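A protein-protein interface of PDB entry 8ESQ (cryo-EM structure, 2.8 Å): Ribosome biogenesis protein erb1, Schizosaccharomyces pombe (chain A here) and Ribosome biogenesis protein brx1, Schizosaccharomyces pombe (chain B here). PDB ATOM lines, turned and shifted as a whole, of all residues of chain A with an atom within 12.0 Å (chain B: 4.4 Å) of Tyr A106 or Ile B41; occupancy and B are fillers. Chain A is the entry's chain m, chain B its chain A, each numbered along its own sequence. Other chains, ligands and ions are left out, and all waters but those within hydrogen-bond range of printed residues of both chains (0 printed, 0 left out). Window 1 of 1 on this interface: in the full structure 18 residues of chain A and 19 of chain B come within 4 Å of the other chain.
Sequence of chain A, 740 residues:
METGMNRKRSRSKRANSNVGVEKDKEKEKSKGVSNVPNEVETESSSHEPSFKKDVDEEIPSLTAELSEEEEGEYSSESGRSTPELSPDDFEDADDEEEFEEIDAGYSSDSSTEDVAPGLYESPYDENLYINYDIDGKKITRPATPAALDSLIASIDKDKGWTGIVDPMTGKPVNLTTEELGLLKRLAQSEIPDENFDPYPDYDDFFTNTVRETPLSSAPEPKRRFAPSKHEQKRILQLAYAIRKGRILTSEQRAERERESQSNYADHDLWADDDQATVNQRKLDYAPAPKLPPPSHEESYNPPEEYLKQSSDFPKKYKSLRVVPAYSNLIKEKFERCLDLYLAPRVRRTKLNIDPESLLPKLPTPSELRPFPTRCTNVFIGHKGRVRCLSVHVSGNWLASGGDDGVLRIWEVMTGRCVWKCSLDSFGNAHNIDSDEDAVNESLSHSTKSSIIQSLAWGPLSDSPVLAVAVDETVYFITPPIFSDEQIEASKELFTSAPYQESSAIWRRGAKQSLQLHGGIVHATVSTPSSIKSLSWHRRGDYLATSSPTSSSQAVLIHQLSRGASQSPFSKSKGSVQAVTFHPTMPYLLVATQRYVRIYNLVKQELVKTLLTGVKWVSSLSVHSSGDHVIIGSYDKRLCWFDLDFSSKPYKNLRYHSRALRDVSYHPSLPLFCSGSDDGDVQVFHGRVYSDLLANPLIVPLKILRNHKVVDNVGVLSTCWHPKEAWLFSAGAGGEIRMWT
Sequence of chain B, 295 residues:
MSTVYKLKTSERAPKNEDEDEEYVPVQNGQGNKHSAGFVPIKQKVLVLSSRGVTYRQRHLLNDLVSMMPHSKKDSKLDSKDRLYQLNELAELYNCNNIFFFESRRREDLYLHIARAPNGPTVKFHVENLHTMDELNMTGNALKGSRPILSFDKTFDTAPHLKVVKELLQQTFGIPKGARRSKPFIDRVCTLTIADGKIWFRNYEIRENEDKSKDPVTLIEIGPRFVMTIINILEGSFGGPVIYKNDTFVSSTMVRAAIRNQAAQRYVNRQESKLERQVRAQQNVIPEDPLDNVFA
The backbone carbonyl oxygen of Tyr A106 is in hydrogen-bond range of the backbone NH of Phe B38 (2.6 Å).
The guanidinium group of Arg B179 lies within hydrogen-bond range of the backbone carbonyl oxygen of Thr A112 (2.4 Å).
O of Ile B41 lies close to O of Asp A103 (3.4 Å).
The backbone carbonyl oxygen (O) of Ala A104 sits close to the backbone carbonyl oxygen (O) of Ile B41 (2.8 Å).
Among the printed residues, pairs that only touch across the chains: Ala A104 with Lys B42 (3.3 Å), Tyr A106 with Ile B41 (3.5 Å), Tyr A106 with Arg B179 (3.5 Å), Ala A104 with Lys B44 (3.5 Å), Glu A113 with Arg B179 (3.6 Å), Tyr A106 with Gly B37 (3.6 Å), Tyr A106 with Lys B44 (3.7 Å), Ser A108 with Phe B38 (3.8 Å), Gly A105 with Pro B40 (3.9 Å), Gly A105 with Lys B44 (3.9 Å), Tyr A106 with Val B39 (3.97 Å), Ser A110 with Lys B44 (3.98 Å) and Asp A114 with Arg B179 (3.99 Å).
Of chain A, only Tyr A106 (2.6 Å) and Ser A108 (3.8 Å) come within 4 Å of Phe B38.
Printed residues of chain A within 4 Å of Val B39: Tyr A106 (3.97 Å).
No residue of chain A comes within 4 Å of Gly B177.
Printed residues of chain B within 4 Å of Asp A114: Arg B179.
Of the printed residues of chain A, Arg B179 touches Tyr A106, Thr A112, Glu A113 and Asp A114.
Of the printed residues of chain B, Ala A104 touches Ile B41 (2.8 Å), Lys B42 (3.3 Å) and Lys B44 (3.5 Å).
Ile A102 touches none of the printed residues of chain B.
The nearest residue of chain A that does not touch Ile B41 is Gly A105 (4.3 Å).
The nearest printed residue of chain B that does not touch Glu A113 is Ala B178 (7.9 Å).
Of the 12 printed residues of chain B, 8 touch a printed residue of chain A.
Among the printed residues, no Asp or Glu carboxylate lies within 4 Å of a Lys or Arg side-chain nitrogen of the other chain.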
ATOM      1  N   GLU A 101     -27.751  33.774  -9.188  1.00  0.00           N
ATOM      2  CA  GLU A 101     -27.051  32.580  -8.727  1.00  0.00           C
ATOM      3  C   GLU A 101     -25.686  32.938  -8.154  1.00  0.00           C
ATOM      4  O   GLU A 101     -25.116  33.978  -8.485  1.00  0.00           O
ATOM      5  CB  GLU A 101     -26.902  31.571  -9.867  1.00  0.00           C
ATOM      6  CG  GLU A 101     -28.210  30.918 -10.289  1.00  0.00           C
ATOM      7  CD  GLU A 101     -29.022  31.782 -11.236  1.00  0.00           C
ATOM      8  OE1 GLU A 101     -28.546  32.878 -11.602  1.00  0.00           O
ATOM      9  OE2 GLU A 101     -30.137  31.364 -11.612  1.00  0.00           O
ATOM     10  N   ILE A 102     -25.165  32.069  -7.291  1.00  0.00           N
ATOM     11  CA  ILE A 102     -23.915  32.318  -6.586  1.00  0.00           C
ATOM     12  C   ILE A 102     -22.867  31.247  -6.845  1.00  0.00           C
ATOM     13  O   ILE A 102     -21.789  31.296  -6.243  1.00  0.00           O
ATOM     14  CB  ILE A 102     -24.154  32.480  -5.071  1.00  0.00           C
ATOM     15  CG1 ILE A 102     -24.784  31.219  -4.488  1.00  0.00           C
ATOM     16  CG2 ILE A 102     -25.042  33.685  -4.802  1.00  0.00           C
ATOM     17  CD1 ILE A 102     -24.932  31.268  -2.994  1.00  0.00           C
ATOM     18  N   ASP A 103     -23.156  30.272  -7.704  1.00  0.00           N
ATOM     19  CA  ASP A 103     -22.241  29.285  -8.266  1.00  0.00           C
ATOM     20  C   ASP A 103     -21.823  28.217  -7.256  1.00  0.00           C
ATOM     21  O   ASP A 103     -21.197  27.235  -7.658  1.00  0.00           O
ATOM     22  CB  ASP A 103     -20.971  29.918  -8.866  1.00  0.00           C
ATOM     23  CG  ASP A 103     -21.286  31.004  -9.874  1.00  0.00           C
ATOM     24  OD1 ASP A 103     -22.346  30.920 -10.528  1.00  0.00           O
ATOM     25  OD2 ASP A 103     -20.477  31.946 -10.007  1.00  0.00           O
ATOM     26  N   ALA A 104     -22.149  28.364  -5.972  1.00  0.00           N
ATOM     27  CA  ALA A 104     -21.846  27.366  -4.951  1.00  0.00           C
ATOM     28  C   ALA A 104     -20.379  26.948  -4.955  1.00  0.00           C
ATOM     29  O   ALA A 104     -20.063  25.780  -4.712  1.00  0.00           O
ATOM     30  CB  ALA A 104     -22.741  26.138  -5.127  1.00  0.00           C
ATOM     31  N   GLY A 105     -19.481  27.890  -5.215  1.00  0.00           N
ATOM     32  CA  GLY A 105     -18.063  27.609  -5.298  1.00  0.00           C
ATOM     33  C   GLY A 105     -17.382  27.612  -3.945  1.00  0.00           C
ATOM     34  O   GLY A 105     -18.024  27.616  -2.892  1.00  0.00           O
ATOM     35  N   TYR A 106     -16.051  27.602  -3.984  1.00  0.00           N
ATOM     36  CA  TYR A 106     -15.214  27.620  -2.787  1.00  0.00           C
ATOM     37  C   TYR A 106     -14.162  28.707  -2.959  1.00  0.00           C
ATOM     38  O   TYR A 106     -13.250  28.567  -3.778  1.00  0.00           O
ATOM     39  CB  TYR A 106     -14.540  26.266  -2.555  1.00  0.00           C
ATOM     40  CG  TYR A 106     -15.400  25.206  -1.907  1.00  0.00           C
ATOM     41  CD1 TYR A 106     -16.639  24.869  -2.425  1.00  0.00           C
ATOM     42  CD2 TYR A 106     -14.953  24.523  -0.787  1.00  0.00           C
ATOM     43  CE1 TYR A 106     -17.419  23.895  -1.833  1.00  0.00           C
ATOM     44  CE2 TYR A 106     -15.723  23.547  -0.192  1.00  0.00           C
ATOM     45  CZ  TYR A 106     -16.953  23.236  -0.718  1.00  0.00           C
ATOM     46  OH  TYR A 106     -17.721  22.262  -0.123  1.00  0.00           O
ATOM     47  N   SER A 107     -14.274  29.783  -2.188  1.00  0.00           N
ATOM     48  CA  SER A 107     -13.228  30.792  -2.211  1.00  0.00           C
ATOM     49  C   SER A 107     -11.939  30.211  -1.642  1.00  0.00           C
ATOM     50  O   SER A 107     -11.956  29.282  -0.830  1.00  0.00           O
ATOM     51  CB  SER A 107     -13.657  32.031  -1.427  1.00  0.00           C
ATOM     52  OG  SER A 107     -14.555  32.823  -2.186  1.00  0.00           O
ATOM     53  N   SER A 108     -10.807  30.763  -2.087  1.00  0.00           N
ATOM     54  CA  SER A 108      -9.514  30.172  -1.759  1.00  0.00           C
ATOM     55  C   SER A 108      -9.216  30.204  -0.266  1.00  0.00           C
ATOM     56  O   SER A 108      -8.322  29.485   0.191  1.00  0.00           O
ATOM     57  CB  SER A 108      -8.400  30.882  -2.529  1.00  0.00           C
ATOM     58  OG  SER A 108      -8.227  32.212  -2.076  1.00  0.00           O
ATOM     59  N   ASP A 109      -9.943  31.011   0.503  1.00  0.00           N
ATOM     60  CA  ASP A 109      -9.735  31.129   1.938  1.00  0.00           C
ATOM     61  C   ASP A 109     -10.795  30.399   2.755  1.00  0.00           C
ATOM     62  O   ASP A 109     -10.912  30.649   3.958  1.00  0.00           O
ATOM     63  CB  ASP A 109      -9.690  32.603   2.340  1.00  0.00           C
ATOM     64  CG  ASP A 109     -10.795  33.416   1.694  1.00  0.00           C
ATOM     65  OD1 ASP A 109     -11.614  32.827   0.958  1.00  0.00           O
ATOM     66  OD2 ASP A 109     -10.846  34.642   1.919  1.00  0.00           O
ATOM     67  N   SER A 110     -11.569  29.510   2.134  1.00  0.00           N
ATOM     68  CA  SER A 110     -12.611  28.799   2.860  1.00  0.00           C
ATOM     69  C   SER A 110     -11.999  27.863   3.894  1.00  0.00           C
ATOM     70  O   SER A 110     -10.979  27.215   3.646  1.00  0.00           O
ATOM     71  CB  SER A 110     -13.494  28.013   1.890  1.00  0.00           C
ATOM     72  OG  SER A 110     -14.728  27.664   2.492  1.00  0.00           O
ATOM     73  N   SER A 111     -12.631  27.796   5.068  1.00  0.00           N
ATOM     74  CA  SER A 111     -12.118  26.975   6.157  1.00  0.00           C
ATOM     75  C   SER A 111     -12.308  25.486   5.915  1.00  0.00           C
ATOM     76  O   SER A 111     -11.753  24.680   6.670  1.00  0.00           O
ATOM     77  CB  SER A 111     -12.788  27.371   7.474  1.00  0.00           C
ATOM     78  OG  SER A 111     -14.186  27.526   7.313  1.00  0.00           O
ATOM     79  N   THR A 112     -13.077  25.102   4.902  1.00  0.00           N
ATOM     80  CA  THR A 112     -13.278  23.701   4.564  1.00  0.00           C
ATOM     81  C   THR A 112     -12.326  23.292   3.447  1.00  0.00           C
ATOM     82  O   THR A 112     -12.219  23.979   2.427  1.00  0.00           O
ATOM     83  CB  THR A 112     -14.731  23.448   4.153  1.00  0.00           C
ATOM     84  OG1 THR A 112     -14.862  22.115   3.643  1.00  0.00           O
ATOM     85  CG2 THR A 112     -15.193  24.457   3.111  1.00  0.00           C
ATOM     86  N   GLU A 113     -11.625  22.181   3.652  1.00  0.00           N
ATOM     87  CA  GLU A 113     -10.652  21.710   2.678  1.00  0.00           C
ATOM     88  C   GLU A 113     -10.490  20.205   2.825  1.00  0.00           C
ATOM     89  O   GLU A 113     -10.857  19.615   3.844  1.00  0.00           O
ATOM     90  CB  GLU A 113      -9.300  22.410   2.849  1.00  0.00           C
ATOM     91  CG  GLU A 113      -8.452  21.846   3.977  1.00  0.00           C
ATOM     92  CD  GLU A 113      -8.867  22.356   5.345  1.00  0.00           C
ATOM     93  OE1 GLU A 113     -10.018  22.811   5.503  1.00  0.00           O
ATOM     94  OE2 GLU A 113      -8.037  22.294   6.271  1.00  0.00           O
ATOM     95  N   ASP A 114      -9.930  19.592   1.788  1.00  0.00           N
ATOM     96  CA  ASP A 114      -9.692  18.159   1.768  1.00  0.00           C
ATOM     97  C   ASP A 114      -8.317  17.835   2.339  1.00  0.00           C
ATOM     98  O   ASP A 114      -7.408  18.671   2.331  1.00  0.00           O
ATOM     99  CB  ASP A 114      -9.804  17.617   0.343  1.00  0.00           C
ATOM    100  CG  ASP A 114      -8.814  18.267  -0.603  1.00  0.00           C
ATOM    101  OD1 ASP A 114      -8.754  19.513  -0.636  1.00  0.00           O
ATOM    102  OD2 ASP A 114      -8.098  17.530  -1.314  1.00  0.00           O
ATOM    103  N   VAL A 115      -8.186  16.612   2.856  1.00  0.00           N
ATOM    104  CA  VAL A 115      -6.919  16.073   3.345  1.00  0.00           C
ATOM    105  C   VAL A 115      -6.477  16.854   4.578  1.00  0.00           C
ATOM    106  O   VAL A 115      -5.710  17.817   4.475  1.00  0.00           O
ATOM    107  CB  VAL A 115      -5.833  16.090   2.251  1.00  0.00           C
ATOM    108  CG1 VAL A 115      -4.530  15.496   2.776  1.00  0.00           C
ATOM    109  CG2 VAL A 115      -6.308  15.338   1.018  1.00  0.00           C
ATOM    110  N   ILE A 134     -10.726   9.427  -4.465  1.00  0.00           N
ATOM    111  CA  ILE A 134     -12.024   9.738  -5.045  1.00  0.00           C
ATOM    112  C   ILE A 134     -12.270   8.806  -6.224  1.00  0.00           C
ATOM    113  O   ILE A 134     -11.332   8.381  -6.912  1.00  0.00           O
ATOM    114  CB  ILE A 134     -12.099  11.219  -5.454  1.00  0.00           C
ATOM    115  CG1 ILE A 134     -13.557  11.671  -5.525  1.00  0.00           C
ATOM    116  CG2 ILE A 134     -11.404  11.458  -6.785  1.00  0.00           C
ATOM    117  CD1 ILE A 134     -14.250  11.685  -4.181  1.00  0.00           C
ATOM    118  N   GLY B  37     -15.220  32.031  -7.030  1.00  0.00           N
ATOM    119  CA  GLY B  37     -14.847  30.860  -6.263  1.00  0.00           C
ATOM    120  C   GLY B  37     -13.850  30.008  -7.013  1.00  0.00           C
ATOM    121  O   GLY B  37     -13.726  30.093  -8.239  1.00  0.00           O
ATOM    122  N   PHE B  38     -13.136  29.184  -6.252  1.00  0.00           N
ATOM    123  CA  PHE B  38     -12.211  28.198  -6.792  1.00  0.00           C
ATOM    124  C   PHE B  38     -12.763  26.803  -6.534  1.00  0.00           C
ATOM    125  O   PHE B  38     -13.364  26.551  -5.486  1.00  0.00           O
ATOM    126  CB  PHE B  38     -10.821  28.332  -6.163  1.00  0.00           C
ATOM    127  CG  PHE B  38     -10.034  29.508  -6.666  1.00  0.00           C
ATOM    128  CD1 PHE B  38     -10.513  30.292  -7.703  1.00  0.00           C
ATOM    129  CD2 PHE B  38      -8.807  29.823  -6.107  1.00  0.00           C
ATOM    130  CE1 PHE B  38      -9.785  31.372  -8.167  1.00  0.00           C
ATOM    131  CE2 PHE B  38      -8.075  30.902  -6.567  1.00  0.00           C
ATOM    132  CZ  PHE B  38      -8.565  31.678  -7.598  1.00  0.00           C
ATOM    133  N   VAL B  39     -12.555  25.902  -7.490  1.00  0.00           N
ATOM    134  CA  VAL B  39     -13.114  24.553  -7.428  1.00  0.00           C
ATOM    135  C   VAL B  39     -14.624  24.671  -7.248  1.00  0.00           C
ATOM    136  O   VAL B  39     -15.136  24.401  -6.154  1.00  0.00           O
ATOM    137  CB  VAL B  39     -12.479  23.723  -6.299  1.00  0.00           C
ATOM    138  CG1 VAL B  39     -12.859  22.254  -6.434  1.00  0.00           C
ATOM    139  CG2 VAL B  39     -10.967  23.887  -6.300  1.00  0.00           C
ATOM    140  N   PRO B  40     -15.368  25.094  -8.267  1.00  0.00           N
ATOM    141  CA  PRO B  40     -16.816  25.260  -8.086  1.00  0.00           C
ATOM    142  C   PRO B  40     -17.555  23.934  -7.999  1.00  0.00           C
ATOM    143  O   PRO B  40     -17.734  23.241  -9.005  1.00  0.00           O
ATOM    144  CB  PRO B  40     -17.234  26.059  -9.327  1.00  0.00           C
ATOM    145  CG  PRO B  40     -16.203  25.741 -10.348  1.00  0.00           C
ATOM    146  CD  PRO B  40     -14.920  25.517  -9.605  1.00  0.00           C
ATOM    147  N   ILE B  41     -17.985  23.574  -6.796  1.00  0.00           N
ATOM    148  CA  ILE B  41     -18.860  22.424  -6.597  1.00  0.00           C
ATOM    149  C   ILE B  41     -20.286  22.822  -6.957  1.00  0.00           C
ATOM    150  O   ILE B  41     -20.688  23.978  -6.794  1.00  0.00           O
ATOM    151  CB  ILE B  41     -18.736  21.900  -5.149  1.00  0.00           C
ATOM    152  CG1 ILE B  41     -17.415  21.145  -4.961  1.00  0.00           C
ATOM    153  CG2 ILE B  41     -19.900  21.018  -4.763  1.00  0.00           C
ATOM    154  CD1 ILE B  41     -16.266  21.992  -4.488  1.00  0.00           C
ATOM    155  N   LYS B  42     -21.054  21.860  -7.479  1.00  0.00           N
ATOM    156  CA  LYS B  42     -22.356  22.176  -8.060  1.00  0.00           C
ATOM    157  C   LYS B  42     -23.299  22.796  -7.035  1.00  0.00           C
ATOM    158  O   LYS B  42     -23.817  23.898  -7.242  1.00  0.00           O
ATOM    159  CB  LYS B  42     -22.976  20.913  -8.657  1.00  0.00           C
ATOM    160  CG  LYS B  42     -24.336  21.131  -9.299  1.00  0.00           C
ATOM    161  CD  LYS B  42     -24.226  21.901 -10.606  1.00  0.00           C
ATOM    162  CE  LYS B  42     -23.669  21.020 -11.713  1.00  0.00           C
ATOM    163  NZ  LYS B  42     -23.701  21.693 -13.041  1.00  0.00           N
ATOM    164  N   GLN B  43     -23.504  22.118  -5.908  1.00  0.00           N
ATOM    165  CA  GLN B  43     -24.477  22.521  -4.897  1.00  0.00           C
ATOM    166  C   GLN B  43     -23.787  22.586  -3.543  1.00  0.00           C
ATOM    167  O   GLN B  43     -23.172  21.606  -3.110  1.00  0.00           O
ATOM    168  CB  GLN B  43     -25.657  21.540  -4.845  1.00  0.00           C
ATOM    169  CG  GLN B  43     -26.615  21.447  -6.065  1.00  0.00           C
ATOM    170  CD  GLN B  43     -27.101  22.776  -6.663  1.00  0.00           C
ATOM    171  OE1 GLN B  43     -26.391  23.775  -6.717  1.00  0.00           O
ATOM    172  NE2 GLN B  43     -28.345  22.767  -7.131  1.00  0.00           N
ATOM    173  N   LYS B  44     -23.892  23.733  -2.879  1.00  0.00           N
ATOM    174  CA  LYS B  44     -23.385  23.907  -1.528  1.00  0.00           C
ATOM    175  C   LYS B  44     -24.530  24.342  -0.626  1.00  0.00           C
ATOM    176  O   LYS B  44     -25.430  25.069  -1.057  1.00  0.00           O
ATOM    177  CB  LYS B  44     -22.245  24.928  -1.487  1.00  0.00           C
ATOM    178  CG  LYS B  44     -21.430  24.888  -0.206  1.00  0.00           C
ATOM    179  CD  LYS B  44     -20.222  25.798  -0.291  1.00  0.00           C
ATOM    180  CE  LYS B  44     -19.428  25.774   1.000  1.00  0.00           C
ATOM    181  NZ  LYS B  44     -18.267  26.699   0.940  1.00  0.00           N
ATOM    182  N   PRO B 175     -23.033  16.457  -4.572  1.00  0.00           N
ATOM    183  CA  PRO B 175     -22.370  16.654  -5.863  1.00  0.00           C
ATOM    184  C   PRO B 175     -20.964  16.078  -5.865  1.00  0.00           C
ATOM    185  O   PRO B 175     -20.293  16.004  -4.833  1.00  0.00           O
ATOM    186  CB  PRO B 175     -22.351  18.178  -6.026  1.00  0.00           C
ATOM    187  CG  PRO B 175     -22.497  18.711  -4.643  1.00  0.00           C
ATOM    188  CD  PRO B 175     -23.319  17.727  -3.885  1.00  0.00           C
ATOM    189  N   GLY B 177     -17.049  15.520  -6.216  1.00  0.00           N
ATOM    190  CA  GLY B 177     -15.912  16.333  -5.850  1.00  0.00           C
ATOM    191  C   GLY B 177     -16.083  17.152  -4.592  1.00  0.00           C
ATOM    192  O   GLY B 177     -15.179  17.925  -4.253  1.00  0.00           O
ATOM    193  N   ALA B 178     -17.209  17.018  -3.896  1.00  0.00           N
ATOM    194  CA  ALA B 178     -17.416  17.757  -2.660  1.00  0.00           C
ATOM    195  C   ALA B 178     -16.379  17.351  -1.622  1.00  0.00           C
ATOM    196  O   ALA B 178     -16.067  16.168  -1.465  1.00  0.00           O
ATOM    197  CB  ALA B 178     -18.826  17.515  -2.127  1.00  0.00           C
ATOM    198  N   ARG B 179     -15.834  18.342  -0.922  1.00  0.00           N
ATOM    199  CA  ARG B 179     -14.819  18.071   0.084  1.00  0.00           C
ATOM    200  C   ARG B 179     -15.419  17.302   1.253  1.00  0.00           C
ATOM    201  O   ARG B 179     -16.578  17.507   1.622  1.00  0.00           O
ATOM    202  CB  ARG B 179     -14.191  19.382   0.556  1.00  0.00           C
ATOM    203  CG  ARG B 179     -13.494  20.136  -0.566  1.00  0.00           C
ATOM    204  CD  ARG B 179     -12.912  21.454  -0.100  1.00  0.00           C
ATOM    205  NE  ARG B 179     -12.269  22.173  -1.193  1.00  0.00           N
ATOM    206  CZ  ARG B 179     -11.683  23.356  -1.072  1.00  0.00           C
ATOM    207  NH1 ARG B 179     -11.641  23.991   0.088  1.00  0.00           N
ATOM    208  NH2 ARG B 179     -11.124  23.915  -2.140  1.00  0.00           N
